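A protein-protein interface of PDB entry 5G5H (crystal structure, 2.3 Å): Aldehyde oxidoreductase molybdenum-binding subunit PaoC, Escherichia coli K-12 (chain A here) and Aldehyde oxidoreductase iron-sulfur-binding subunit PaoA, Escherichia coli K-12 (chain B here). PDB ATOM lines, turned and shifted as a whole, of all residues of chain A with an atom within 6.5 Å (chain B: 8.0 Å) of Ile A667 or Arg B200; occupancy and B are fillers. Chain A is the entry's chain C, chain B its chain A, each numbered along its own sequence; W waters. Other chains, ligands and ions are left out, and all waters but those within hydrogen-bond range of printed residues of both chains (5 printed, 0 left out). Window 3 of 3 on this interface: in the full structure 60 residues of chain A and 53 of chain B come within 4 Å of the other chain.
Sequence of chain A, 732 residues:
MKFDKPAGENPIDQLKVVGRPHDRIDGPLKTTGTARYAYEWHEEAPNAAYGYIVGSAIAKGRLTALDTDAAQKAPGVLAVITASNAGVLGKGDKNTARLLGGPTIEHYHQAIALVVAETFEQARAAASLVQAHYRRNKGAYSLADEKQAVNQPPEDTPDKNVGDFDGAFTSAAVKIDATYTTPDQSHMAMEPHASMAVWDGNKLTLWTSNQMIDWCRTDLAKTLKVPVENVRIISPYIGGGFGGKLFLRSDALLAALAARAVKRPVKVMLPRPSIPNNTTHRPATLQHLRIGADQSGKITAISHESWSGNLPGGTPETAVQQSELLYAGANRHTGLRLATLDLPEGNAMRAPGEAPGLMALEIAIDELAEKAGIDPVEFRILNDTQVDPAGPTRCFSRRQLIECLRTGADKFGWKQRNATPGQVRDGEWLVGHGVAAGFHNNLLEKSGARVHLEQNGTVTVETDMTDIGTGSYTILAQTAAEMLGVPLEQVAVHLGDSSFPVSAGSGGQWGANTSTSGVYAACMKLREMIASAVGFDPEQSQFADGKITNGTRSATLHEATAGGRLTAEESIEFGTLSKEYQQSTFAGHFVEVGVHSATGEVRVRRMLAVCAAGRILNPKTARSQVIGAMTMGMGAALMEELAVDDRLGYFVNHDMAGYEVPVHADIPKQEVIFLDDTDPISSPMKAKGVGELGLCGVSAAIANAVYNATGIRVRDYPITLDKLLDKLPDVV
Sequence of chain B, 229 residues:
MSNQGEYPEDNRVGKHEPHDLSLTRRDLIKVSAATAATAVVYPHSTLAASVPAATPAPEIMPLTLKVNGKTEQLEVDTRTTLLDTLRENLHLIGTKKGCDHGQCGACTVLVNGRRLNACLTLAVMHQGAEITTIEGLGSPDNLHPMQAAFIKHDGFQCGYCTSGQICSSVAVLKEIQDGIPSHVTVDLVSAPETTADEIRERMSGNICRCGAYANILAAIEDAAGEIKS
Among the printed residues, pairs that only touch across the chains: His A664 with Arg B200 (3.1 Å), His A664 with Met B203 (3.2 Å), His A664 with Tyr B213 (3.4 Å), His A664 with Asn B206 (3.5 Å), Ile A667 with Tyr B213 (3.5 Å), Val A663 with Tyr B213 (3.6 Å), Gln A670 with Ala B214 (3.6 Å), Ala A665 with Arg B200 (3.6 Å), Val A663 with Ser B204 (3.7 Å), His A664 with Ser B204 (3.7 Å), Thr A631 with Gly B211 (3.8 Å) and Thr A631 with Tyr B213 (3.9 Å).
Of the printed residues of chain B, Ile A667 touches Arg B200 and Tyr B213. Arg B200 touches just these residues of chain A: His A664, Ala A665 and Ile A667. No residue of chain B comes within 4 Å of Pro A668. Of the printed residues of chain A, Ala B214 touches Gln A670. Of the printed residues of chain A, Gly B211 touches Thr A631. Of the printed residues of chain A, Tyr B213 touches Thr A631, Pro A662, Val A663, His A664 and Ile A667. Printed residues of chain B within 4 Å of Ala A665: Arg B200 and Ser B204. Asp B197 touches none of the printed residues of chain A. Glu B201 touches none of the printed residues of chain A.
N of Val A663 lies within hydrogen-bond range of OD2 of Asp A666, 3.0 Å away. The backbone NH of Cys B208 sits at hydrogen-bond distance from the side-chain hydroxyl of Tyr B213 (2.9 Å). The backbone carbonyl oxygen of Arg B200 sits at hydrogen-bond distance from the side-chain hydroxyl of Ser B204 (2.8 Å). The side-chain sulfur (SG) of Cys B208 lies close to the backbone NH (N) of Gly B211 (3.4 Å). OG1 of Thr A631 sits at hydrogen-bond distance from NE2 of Gln A670, at 3.2 Å.
Of the 12 printed residues of chain A, 7 touch a printed residue of chain B. Along chain A the printed residues that touch a printed residue of chain B span positions 631 to 670. Of the 25 printed residues of chain B, 7 touch a printed residue of chain A.
O of Pro A662 is in hydrogen-bond range of OH of Tyr B213. OG of Ser B204 lies within hydrogen-bond range of N of Ala A665, at 2.8 Å. NE of Arg B200 lies within hydrogen-bond range of O of Ile A667, 3.2 Å away.
Water W4 lies within hydrogen-bond range of the side-chain amide oxygen (OE1) of Gln A670, the backbone NH (N) of Ala B214 and the backbone carbonyl oxygen (O) of Gly B211. Water W2 lies within hydrogen-bond range of O of Asn B206 (2.8 Å), O of Ser B204 (2.9 Å), N of His A664 (2.9 Å) and OH of Tyr B213 (3.4 Å). Water W3 lies within hydrogen-bond range of the backbone carbonyl oxygen (O) of Pro A662 (2.8 Å) and the backbone carbonyl oxygen (O) of Cys B208 (2.9 Å). Water W1 bridges NE of Arg B200 and O of Ile A667. Water W5 lies within hydrogen-bond range of the backbone carbonyl oxygen of Ala A665 (2.9 Å) and the side-chain carboxylate of Asp B197 (3.3 Å).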
ATOM      1  N   VAL A 604     -18.065 -28.108 -26.418  1.00  0.00           N
ATOM      2  CA  VAL A 604     -19.219 -28.702 -25.766  1.00  0.00           C
ATOM      3  C   VAL A 604     -20.452 -27.869 -26.119  1.00  0.00           C
ATOM      4  O   VAL A 604     -20.460 -26.652 -25.954  1.00  0.00           O
ATOM      5  CB  VAL A 604     -19.040 -28.825 -24.240  1.00  0.00           C
ATOM      6  CG1 VAL A 604     -20.183 -29.630 -23.640  1.00  0.00           C
ATOM      7  CG2 VAL A 604     -17.720 -29.507 -23.929  1.00  0.00           C
ATOM      8  N   THR A 631     -18.144 -27.384 -15.376  1.00  0.00           N
ATOM      9  CA  THR A 631     -17.115 -26.556 -16.000  1.00  0.00           C
ATOM     10  C   THR A 631     -15.698 -27.105 -15.736  1.00  0.00           C
ATOM     11  O   THR A 631     -14.896 -27.212 -16.649  1.00  0.00           O
ATOM     12  CB  THR A 631     -17.264 -25.082 -15.563  1.00  0.00           C
ATOM     13  OG1 THR A 631     -18.540 -24.606 -15.977  1.00  0.00           O
ATOM     14  CG2 THR A 631     -16.191 -24.199 -16.193  1.00  0.00           C
ATOM     15  N   MET A 634     -15.166 -30.134 -17.773  1.00  0.00           N
ATOM     16  CA  MET A 634     -14.811 -29.780 -19.139  1.00  0.00           C
ATOM     17  C   MET A 634     -13.305 -29.482 -19.281  1.00  0.00           C
ATOM     18  O   MET A 634     -12.655 -29.885 -20.273  1.00  0.00           O
ATOM     19  CB  MET A 634     -15.636 -28.591 -19.616  1.00  0.00           C
ATOM     20  CG  MET A 634     -15.805 -28.568 -21.111  1.00  0.00           C
ATOM     21  SD  MET A 634     -16.241 -26.959 -21.750  1.00  0.00           S
ATOM     22  CE  MET A 634     -17.872 -26.715 -21.053  1.00  0.00           C
ATOM     23  N   PRO A 662     -11.223 -23.484 -18.416  1.00  0.00           N
ATOM     24  CA  PRO A 662     -12.293 -22.960 -19.288  1.00  0.00           C
ATOM     25  C   PRO A 662     -12.676 -21.477 -19.137  1.00  0.00           C
ATOM     26  O   PRO A 662     -12.655 -20.939 -18.043  1.00  0.00           O
ATOM     27  CB  PRO A 662     -13.481 -23.858 -18.930  1.00  0.00           C
ATOM     28  CG  PRO A 662     -12.835 -25.142 -18.529  1.00  0.00           C
ATOM     29  CD  PRO A 662     -11.661 -24.706 -17.715  1.00  0.00           C
ATOM     30  N   VAL A 663     -13.035 -20.865 -20.262  1.00  0.00           N
ATOM     31  CA  VAL A 663     -13.464 -19.467 -20.328  1.00  0.00           C
ATOM     32  C   VAL A 663     -14.927 -19.368 -20.729  1.00  0.00           C
ATOM     33  O   VAL A 663     -15.508 -20.353 -21.188  1.00  0.00           O
ATOM     34  CB  VAL A 663     -12.620 -18.647 -21.331  1.00  0.00           C
ATOM     35  CG1 VAL A 663     -11.176 -18.550 -20.845  1.00  0.00           C
ATOM     36  CG2 VAL A 663     -12.681 -19.228 -22.746  1.00  0.00           C
ATOM     37  N   HIS A 664     -15.506 -18.173 -20.583  1.00  0.00           N
ATOM     38  CA  HIS A 664     -16.902 -17.922 -20.987  1.00  0.00           C
ATOM     39  C   HIS A 664     -17.259 -18.547 -22.346  1.00  0.00           C
ATOM     40  O   HIS A 664     -18.267 -19.251 -22.451  1.00  0.00           O
ATOM     41  CB  HIS A 664     -17.211 -16.426 -21.063  1.00  0.00           C
ATOM     42  CG  HIS A 664     -17.679 -15.816 -19.783  1.00  0.00           C
ATOM     43  ND1 HIS A 664     -19.006 -15.812 -19.411  1.00  0.00           N
ATOM     44  CD2 HIS A 664     -17.017 -15.116 -18.823  1.00  0.00           C
ATOM     45  CE1 HIS A 664     -19.140 -15.151 -18.273  1.00  0.00           C
ATOM     46  NE2 HIS A 664     -17.948 -14.717 -17.894  1.00  0.00           N
ATOM     47  N   ALA A 665     -16.426 -18.298 -23.365  1.00  0.00           N
ATOM     48  CA  ALA A 665     -16.649 -18.831 -24.737  1.00  0.00           C
ATOM     49  C   ALA A 665     -16.809 -20.354 -24.858  1.00  0.00           C
ATOM     50  O   ALA A 665     -17.463 -20.816 -25.789  1.00  0.00           O
ATOM     51  CB  ALA A 665     -15.559 -18.367 -25.679  1.00  0.00           C
ATOM     52  N   ASP A 666     -16.217 -21.109 -23.929  1.00  0.00           N
ATOM     53  CA  ASP A 666     -16.338 -22.574 -23.876  1.00  0.00           C
ATOM     54  C   ASP A 666     -17.679 -23.144 -23.370  1.00  0.00           C
ATOM     55  O   ASP A 666     -17.952 -24.337 -23.554  1.00  0.00           O
ATOM     56  CB  ASP A 666     -15.238 -23.154 -22.970  1.00  0.00           C
ATOM     57  CG  ASP A 666     -13.861 -22.953 -23.529  1.00  0.00           C
ATOM     58  OD1 ASP A 666     -13.679 -23.243 -24.732  1.00  0.00           O
ATOM     59  OD2 ASP A 666     -12.962 -22.508 -22.775  1.00  0.00           O
ATOM     60  N   ILE A 667     -18.498 -22.322 -22.729  1.00  0.00           N
ATOM     61  CA  ILE A 667     -19.543 -22.835 -21.875  1.00  0.00           C
ATOM     62  C   ILE A 667     -20.839 -22.972 -22.648  1.00  0.00           C
ATOM     63  O   ILE A 667     -21.349 -21.988 -23.163  1.00  0.00           O
ATOM     64  CB  ILE A 667     -19.758 -21.934 -20.648  1.00  0.00           C
ATOM     65  CG1 ILE A 667     -18.426 -21.645 -19.951  1.00  0.00           C
ATOM     66  CG2 ILE A 667     -20.742 -22.570 -19.675  1.00  0.00           C
ATOM     67  CD1 ILE A 667     -17.623 -22.872 -19.565  1.00  0.00           C
ATOM     68  N   PRO A 668     -21.376 -24.196 -22.735  1.00  0.00           N
ATOM     69  CA  PRO A 668     -22.675 -24.404 -23.360  1.00  0.00           C
ATOM     70  C   PRO A 668     -23.789 -24.153 -22.368  1.00  0.00           C
ATOM     71  O   PRO A 668     -23.553 -23.680 -21.242  1.00  0.00           O
ATOM     72  CB  PRO A 668     -22.645 -25.885 -23.709  1.00  0.00           C
ATOM     73  CG  PRO A 668     -21.876 -26.489 -22.589  1.00  0.00           C
ATOM     74  CD  PRO A 668     -20.845 -25.461 -22.189  1.00  0.00           C
ATOM     75  N   LYS A 669     -24.997 -24.476 -22.791  1.00  0.00           N
ATOM     76  CA  LYS A 669     -26.100 -24.615 -21.872  1.00  0.00           C
ATOM     77  C   LYS A 669     -25.751 -25.775 -20.937  1.00  0.00           C
ATOM     78  O   LYS A 669     -25.233 -26.818 -21.374  1.00  0.00           O
ATOM     79  CB  LYS A 669     -27.392 -24.911 -22.623  1.00  0.00           C
ATOM     80  CG  LYS A 669     -28.628 -24.835 -21.746  1.00  0.00           C
ATOM     81  CD  LYS A 669     -29.879 -25.218 -22.511  1.00  0.00           C
ATOM     82  CE  LYS A 669     -29.839 -26.674 -22.916  1.00  0.00           C
ATOM     83  NZ  LYS A 669     -31.217 -27.146 -23.155  1.00  0.00           N
ATOM     84  N   GLN A 670     -26.007 -25.548 -19.654  1.00  0.00           N
ATOM     85  CA  GLN A 670     -25.719 -26.493 -18.581  1.00  0.00           C
ATOM     86  C   GLN A 670     -26.963 -26.612 -17.726  1.00  0.00           C
ATOM     87  O   GLN A 670     -27.401 -25.623 -17.124  1.00  0.00           O
ATOM     88  CB  GLN A 670     -24.554 -25.984 -17.728  1.00  0.00           C
ATOM     89  CG  GLN A 670     -23.191 -26.165 -18.372  1.00  0.00           C
ATOM     90  CD  GLN A 670     -22.072 -25.401 -17.670  1.00  0.00           C
ATOM     91  OE1 GLN A 670     -22.312 -24.416 -16.981  1.00  0.00           O
ATOM     92  NE2 GLN A 670     -20.831 -25.841 -17.881  1.00  0.00           N
ATOM     93  N   VAL B 172     -18.961  -4.107 -21.466  1.00  0.00           N
ATOM     94  CA  VAL B 172     -19.292  -4.947 -22.631  1.00  0.00           C
ATOM     95  C   VAL B 172     -20.588  -4.521 -23.306  1.00  0.00           C
ATOM     96  O   VAL B 172     -20.663  -4.511 -24.536  1.00  0.00           O
ATOM     97  CB  VAL B 172     -19.344  -6.455 -22.254  1.00  0.00           C
ATOM     98  CG1 VAL B 172     -20.105  -7.300 -23.282  1.00  0.00           C
ATOM     99  CG2 VAL B 172     -17.934  -6.990 -22.121  1.00  0.00           C
ATOM    100  N   ILE B 176     -20.938  -3.029 -27.231  1.00  0.00           N
ATOM    101  CA  ILE B 176     -21.953  -3.481 -28.193  1.00  0.00           C
ATOM    102  C   ILE B 176     -22.781  -2.277 -28.697  1.00  0.00           C
ATOM    103  O   ILE B 176     -22.921  -2.096 -29.911  1.00  0.00           O
ATOM    104  CB  ILE B 176     -22.857  -4.609 -27.603  1.00  0.00           C
ATOM    105  CG1 ILE B 176     -22.028  -5.875 -27.319  1.00  0.00           C
ATOM    106  CG2 ILE B 176     -24.003  -4.971 -28.550  1.00  0.00           C
ATOM    107  CD1 ILE B 176     -22.637  -6.817 -26.296  1.00  0.00           C
ATOM    108  N   SER B 182     -16.742  -8.219 -32.669  1.00  0.00           N
ATOM    109  CA  SER B 182     -15.994  -9.227 -31.917  1.00  0.00           C
ATOM    110  C   SER B 182     -15.619 -10.404 -32.801  1.00  0.00           C
ATOM    111  O   SER B 182     -15.886 -10.413 -33.997  1.00  0.00           O
ATOM    112  CB  SER B 182     -16.782  -9.706 -30.692  1.00  0.00           C
ATOM    113  OG  SER B 182     -17.630 -10.801 -30.997  1.00  0.00           O
ATOM    114  N   VAL B 184     -16.883 -13.314 -32.865  1.00  0.00           N
ATOM    115  CA  VAL B 184     -18.057 -14.080 -33.282  1.00  0.00           C
ATOM    116  C   VAL B 184     -19.045 -13.258 -34.106  1.00  0.00           C
ATOM    117  O   VAL B 184     -20.079 -13.775 -34.507  1.00  0.00           O
ATOM    118  CB  VAL B 184     -18.774 -14.705 -32.053  1.00  0.00           C
ATOM    119  CG1 VAL B 184     -17.760 -15.385 -31.138  1.00  0.00           C
ATOM    120  CG2 VAL B 184     -19.591 -13.678 -31.260  1.00  0.00           C
ATOM    121  N   THR B 195     -26.290 -10.714 -28.447  1.00  0.00           N
ATOM    122  CA  THR B 195     -26.613 -12.129 -28.364  1.00  0.00           C
ATOM    123  C   THR B 195     -25.821 -12.770 -27.235  1.00  0.00           C
ATOM    124  O   THR B 195     -24.876 -12.181 -26.695  1.00  0.00           O
ATOM    125  CB  THR B 195     -26.296 -12.869 -29.678  1.00  0.00           C
ATOM    126  OG1 THR B 195     -24.876 -12.918 -29.885  1.00  0.00           O
ATOM    127  CG2 THR B 195     -26.954 -12.190 -30.855  1.00  0.00           C
ATOM    128  N   ALA B 196     -26.225 -13.984 -26.889  1.00  0.00           N
ATOM    129  CA  ALA B 196     -25.511 -14.792 -25.922  1.00  0.00           C
ATOM    130  C   ALA B 196     -24.109 -15.146 -26.455  1.00  0.00           C
ATOM    131  O   ALA B 196     -23.134 -15.159 -25.699  1.00  0.00           O
ATOM    132  CB  ALA B 196     -26.302 -16.050 -25.602  1.00  0.00           C
ATOM    133  N   ASP B 197     -24.006 -15.404 -27.757  1.00  0.00           N
ATOM    134  CA  ASP B 197     -22.729 -15.755 -28.351  1.00  0.00           C
ATOM    135  C   ASP B 197     -21.745 -14.577 -28.218  1.00  0.00           C
ATOM    136  O   ASP B 197     -20.597 -14.757 -27.819  1.00  0.00           O
ATOM    137  CB  ASP B 197     -22.920 -16.168 -29.815  1.00  0.00           C
ATOM    138  CG  ASP B 197     -21.912 -17.230 -30.280  1.00  0.00           C
ATOM    139  OD1 ASP B 197     -21.072 -17.713 -29.476  1.00  0.00           O
ATOM    140  OD2 ASP B 197     -21.970 -17.597 -31.479  1.00  0.00           O
ATOM    141  N   GLU B 198     -22.223 -13.374 -28.528  1.00  0.00           N
ATOM    142  CA  GLU B 198     -21.418 -12.149 -28.412  1.00  0.00           C
ATOM    143  C   GLU B 198     -20.929 -11.858 -26.985  1.00  0.00           C
ATOM    144  O   GLU B 198     -19.753 -11.551 -26.788  1.00  0.00           O
ATOM    145  CB  GLU B 198     -22.202 -10.956 -28.971  1.00  0.00           C
ATOM    146  CG  GLU B 198     -22.326 -10.989 -30.489  1.00  0.00           C
ATOM    147  CD  GLU B 198     -21.203 -10.276 -31.227  1.00  0.00           C
ATOM    148  OE1 GLU B 198     -20.141  -9.994 -30.617  1.00  0.00           O
ATOM    149  OE2 GLU B 198     -21.386  -9.998 -32.438  1.00  0.00           O
ATOM    150  N   ILE B 199     -21.814 -11.992 -25.997  1.00  0.00           N
ATOM    151  CA  ILE B 199     -21.459 -11.680 -24.607  1.00  0.00           C
ATOM    152  C   ILE B 199     -20.382 -12.626 -24.089  1.00  0.00           C
ATOM    153  O   ILE B 199     -19.422 -12.194 -23.434  1.00  0.00           O
ATOM    154  CB  ILE B 199     -22.679 -11.728 -23.664  1.00  0.00           C
ATOM    155  CG1 ILE B 199     -23.648 -10.582 -23.986  1.00  0.00           C
ATOM    156  CG2 ILE B 199     -22.245 -11.641 -22.204  1.00  0.00           C
ATOM    157  CD1 ILE B 199     -25.068 -10.815 -23.494  1.00  0.00           C
ATOM    158  N   ARG B 200     -20.570 -13.908 -24.356  1.00  0.00           N
ATOM    159  CA  ARG B 200     -19.602 -14.937 -23.977  1.00  0.00           C
ATOM    160  C   ARG B 200     -18.188 -14.637 -24.446  1.00  0.00           C
ATOM    161  O   ARG B 200     -17.235 -14.754 -23.673  1.00  0.00           O
ATOM    162  CB  ARG B 200     -19.991 -16.267 -24.592  1.00  0.00           C
ATOM    163  CG  ARG B 200     -21.042 -17.020 -23.839  1.00  0.00           C
ATOM    164  CD  ARG B 200     -21.176 -18.388 -24.454  1.00  0.00           C
ATOM    165  NE  ARG B 200     -22.342 -19.058 -23.923  1.00  0.00           N
ATOM    166  CZ  ARG B 200     -23.508 -19.216 -24.552  1.00  0.00           C
ATOM    167  NH1 ARG B 200     -23.731 -18.768 -25.802  1.00  0.00           N
ATOM    168  NH2 ARG B 200     -24.473 -19.856 -23.904  1.00  0.00           N
ATOM    169  N   GLU B 201     -18.068 -14.294 -25.726  1.00  0.00           N
ATOM    170  CA  GLU B 201     -16.761 -14.011 -26.323  1.00  0.00           C
ATOM    171  C   GLU B 201     -16.151 -12.761 -25.689  1.00  0.00           C
ATOM    172  O   GLU B 201     -15.007 -12.767 -25.243  1.00  0.00           O
ATOM    173  CB  GLU B 201     -16.879 -13.871 -27.852  1.00  0.00           C
ATOM    174  CG  GLU B 201     -15.738 -13.142 -28.563  1.00  0.00           C
ATOM    175  CD  GLU B 201     -14.356 -13.723 -28.310  1.00  0.00           C
ATOM    176  OE1 GLU B 201     -14.237 -14.903 -27.935  1.00  0.00           O
ATOM    177  OE2 GLU B 201     -13.368 -12.988 -28.517  1.00  0.00           O
ATOM    178  N   ARG B 202     -16.954 -11.711 -25.628  1.00  0.00           N
ATOM    179  CA  ARG B 202     -16.522 -10.421 -25.097  1.00  0.00           C
ATOM    180  C   ARG B 202     -16.175 -10.495 -23.608  1.00  0.00           C
ATOM    181  O   ARG B 202     -15.357  -9.714 -23.121  1.00  0.00           O
ATOM    182  CB  ARG B 202     -17.612  -9.381 -25.352  1.00  0.00           C
ATOM    183  CG  ARG B 202     -17.856  -9.079 -26.825  1.00  0.00           C
ATOM    184  CD  ARG B 202     -19.133  -8.274 -27.020  1.00  0.00           C
ATOM    185  NE  ARG B 202     -19.483  -8.099 -28.431  1.00  0.00           N
ATOM    186  CZ  ARG B 202     -19.103  -7.094 -29.223  1.00  0.00           C
ATOM    187  NH1 ARG B 202     -18.312  -6.103 -28.794  1.00  0.00           N
ATOM    188  NH2 ARG B 202     -19.522  -7.089 -30.488  1.00  0.00           N
ATOM    189  N   MET B 203     -16.803 -11.436 -22.899  1.00  0.00           N
ATOM    190  CA  MET B 203     -16.487 -11.721 -21.493  1.00  0.00           C
ATOM    191  C   MET B 203     -15.400 -12.777 -21.265  1.00  0.00           C
ATOM    192  O   MET B 203     -15.037 -13.018 -20.116  1.00  0.00           O
ATOM    193  CB  MET B 203     -17.754 -12.145 -20.741  1.00  0.00           C
ATOM    194  CG  MET B 203     -18.804 -11.048 -20.569  1.00  0.00           C
ATOM    195  SD  MET B 203     -18.388  -9.655 -19.475  1.00  0.00           S
ATOM    196  CE  MET B 203     -17.902 -10.492 -17.959  1.00  0.00           C
ATOM    197  N   SER B 204     -14.876 -13.412 -22.312  1.00  0.00           N
ATOM    198  CA  SER B 204     -13.926 -14.521 -22.116  1.00  0.00           C
ATOM    199  C   SER B 204     -12.601 -14.108 -21.439  1.00  0.00           C
ATOM    200  O   SER B 204     -11.892 -14.953 -20.892  1.00  0.00           O
ATOM    201  CB  SER B 204     -13.659 -15.260 -23.418  1.00  0.00           C
ATOM    202  OG  SER B 204     -14.771 -16.057 -23.778  1.00  0.00           O
ATOM    203  N   GLY B 205     -12.291 -12.813 -21.450  1.00  0.00           N
ATOM    204  CA  GLY B 205     -11.222 -12.278 -20.639  1.00  0.00           C
ATOM    205  C   GLY B 205     -11.449 -12.159 -19.138  1.00  0.00           C
ATOM    206  O   GLY B 205     -10.590 -11.636 -18.452  1.00  0.00           O
ATOM    207  N   ASN B 206     -12.590 -12.612 -18.620  1.00  0.00           N
ATOM    208  CA  ASN B 206     -12.786 -12.725 -17.187  1.00  0.00           C
ATOM    209  C   ASN B 206     -12.957 -14.176 -16.780  1.00  0.00           C
ATOM    210  O   ASN B 206     -14.021 -14.784 -17.029  1.00  0.00           O
ATOM    211  CB  ASN B 206     -13.985 -11.902 -16.737  1.00  0.00           C
ATOM    212  CG  ASN B 206     -13.746 -10.419 -16.883  1.00  0.00           C
ATOM    213  OD1 ASN B 206     -13.929  -9.857 -17.966  1.00  0.00           O
ATOM    214  ND2 ASN B 206     -13.326  -9.770 -15.796  1.00  0.00           N
ATOM    215  N   CYS B 208     -13.473 -17.403 -14.388  1.00  0.00           N
ATOM    216  CA  CYS B 208     -14.115 -17.903 -13.179  1.00  0.00           C
ATOM    217  C   CYS B 208     -13.768 -19.379 -13.016  1.00  0.00           C
ATOM    218  O   CYS B 208     -14.254 -20.233 -13.779  1.00  0.00           O
ATOM    219  CB  CYS B 208     -15.636 -17.720 -13.236  1.00  0.00           C
ATOM    220  SG  CYS B 208     -16.479 -18.187 -11.707  1.00  0.00           S
ATOM    221  N   GLY B 211     -16.591 -21.596 -11.963  1.00  0.00           N
ATOM    222  CA  GLY B 211     -17.418 -22.024 -13.064  1.00  0.00           C
ATOM    223  C   GLY B 211     -18.835 -21.515 -12.956  1.00  0.00           C
ATOM    224  O   GLY B 211     -19.787 -22.245 -13.279  1.00  0.00           O
ATOM    225  N   ALA B 212     -18.968 -20.254 -12.534  1.00  0.00           N
ATOM    226  CA  ALA B 212     -20.267 -19.593 -12.418  1.00  0.00           C
ATOM    227  C   ALA B 212     -20.815 -19.072 -13.756  1.00  0.00           C
ATOM    228  O   ALA B 212     -21.936 -18.582 -13.807  1.00  0.00           O
ATOM    229  CB  ALA B 212     -20.178 -18.448 -11.414  1.00  0.00           C
ATOM    230  N   TYR B 213     -19.996 -19.153 -14.802  1.00  0.00           N
ATOM    231  CA  TYR B 213     -20.283 -18.692 -16.160  1.00  0.00           C
ATOM    232  C   TYR B 213     -21.731 -18.716 -16.649  1.00  0.00           C
ATOM    233  O   TYR B 213     -22.217 -17.697 -17.127  1.00  0.00           O
ATOM    234  CB  TYR B 213     -19.443 -19.504 -17.161  1.00  0.00           C
ATOM    235  CG  TYR B 213     -17.934 -19.329 -17.054  1.00  0.00           C
ATOM    236  CD1 TYR B 213     -17.359 -18.072 -17.117  1.00  0.00           C
ATOM    237  CD2 TYR B 213     -17.097 -20.429 -16.922  1.00  0.00           C
ATOM    238  CE1 TYR B 213     -15.998 -17.907 -17.032  1.00  0.00           C
ATOM    239  CE2 TYR B 213     -15.729 -20.284 -16.847  1.00  0.00           C
ATOM    240  CZ  TYR B 213     -15.183 -19.012 -16.902  1.00  0.00           C
ATOM    241  OH  TYR B 213     -13.837 -18.835 -16.826  1.00  0.00           O
ATOM    242  N   ALA B 214     -22.404 -19.862 -16.572  1.00  0.00           N
ATOM    243  CA  ALA B 214     -23.763 -19.960 -17.121  1.00  0.00           C
ATOM    244  C   ALA B 214     -24.675 -18.987 -16.408  1.00  0.00           C
ATOM    245  O   ALA B 214     -25.489 -18.340 -17.045  1.00  0.00           O
ATOM    246  CB  ALA B 214     -24.319 -21.382 -17.039  1.00  0.00           C
ATOM    247  N   ASN B 215     -24.525 -18.888 -15.093  1.00  0.00           N
ATOM    248  CA  ASN B 215     -25.243 -17.900 -14.296  1.00  0.00           C
ATOM    249  C   ASN B 215     -24.837 -16.452 -14.550  1.00  0.00           C
ATOM    250  O   ASN B 215     -25.684 -15.568 -14.517  1.00  0.00           O
ATOM    251  CB  ASN B 215     -25.094 -18.212 -12.808  1.00  0.00           C
ATOM    252  CG  ASN B 215     -25.820 -19.474 -12.409  1.00  0.00           C
ATOM    253  OD1 ASN B 215     -26.570 -20.043 -13.199  1.00  0.00           O
ATOM    254  ND2 ASN B 215     -25.605 -19.919 -11.176  1.00  0.00           N
ATOM    255  N   LEU B 217     -23.792 -15.276 -17.473  1.00  0.00           N
ATOM    256  CA  LEU B 217     -24.528 -14.995 -18.697  1.00  0.00           C
ATOM    257  C   LEU B 217     -25.984 -14.637 -18.401  1.00  0.00           C
ATOM    258  O   LEU B 217     -26.481 -13.679 -18.965  1.00  0.00           O
ATOM    259  CB  LEU B 217     -24.497 -16.177 -19.671  1.00  0.00           C
ATOM    260  CG  LEU B 217     -25.206 -15.943 -21.021  1.00  0.00           C
ATOM    261  CD1 LEU B 217     -24.485 -14.853 -21.813  1.00  0.00           C
ATOM    262  CD2 LEU B 217     -25.320 -17.230 -21.831  1.00  0.00           C
ATOM    263  N   ILE B 220     -26.295 -11.092 -17.022  1.00  0.00           N
ATOM    264  CA  ILE B 220     -26.019 -10.025 -17.976  1.00  0.00           C
ATOM    265  C   ILE B 220     -27.200  -9.814 -18.933  1.00  0.00           C
ATOM    266  O   ILE B 220     -27.634  -8.670 -19.147  1.00  0.00           O
ATOM    267  CB  ILE B 220     -24.692 -10.265 -18.719  1.00  0.00           C
ATOM    268  CG1 ILE B 220     -23.538 -10.250 -17.701  1.00  0.00           C
ATOM    269  CG2 ILE B 220     -24.474  -9.175 -19.767  1.00  0.00           C
ATOM    270  CD1 ILE B 220     -22.198 -10.694 -18.249  1.00  0.00           C
ATOM    271  N   GLU B 221     -27.729 -10.914 -19.470  1.00  0.00           N
ATOM    272  CA  GLU B 221     -28.921 -10.869 -20.326  1.00  0.00           C
ATOM    273  C   GLU B 221     -30.146 -10.281 -19.622  1.00  0.00           C
ATOM    274  O   GLU B 221     -30.943  -9.558 -20.239  1.00  0.00           O
ATOM    275  CB  GLU B 221     -29.242 -12.257 -20.870  1.00  0.00           C
ATOM    276  CG  GLU B 221     -28.263 -12.693 -21.946  1.00  0.00           C
ATOM    277  CD  GLU B 221     -28.555 -14.078 -22.473  1.00  0.00           C
ATOM    278  OE1 GLU B 221     -28.500 -15.029 -21.661  1.00  0.00           O
ATOM    279  OE2 GLU B 221     -28.830 -14.212 -23.689  1.00  0.00           O
HETATM  280  O   HOH W   1     -22.468 -19.622 -21.108  1.00  0.00           O
HETATM  281  O   HOH W   2     -13.676 -16.423 -19.223  1.00  0.00           O
HETATM  282  O   HOH W   3     -12.710 -22.081 -15.443  1.00  0.00           O
HETATM  283  O   HOH W   4     -21.186 -22.293 -15.870  1.00  0.00           O
HETATM  284  O   HOH W   5     -19.758 -19.563 -27.066  1.00  0.00           O
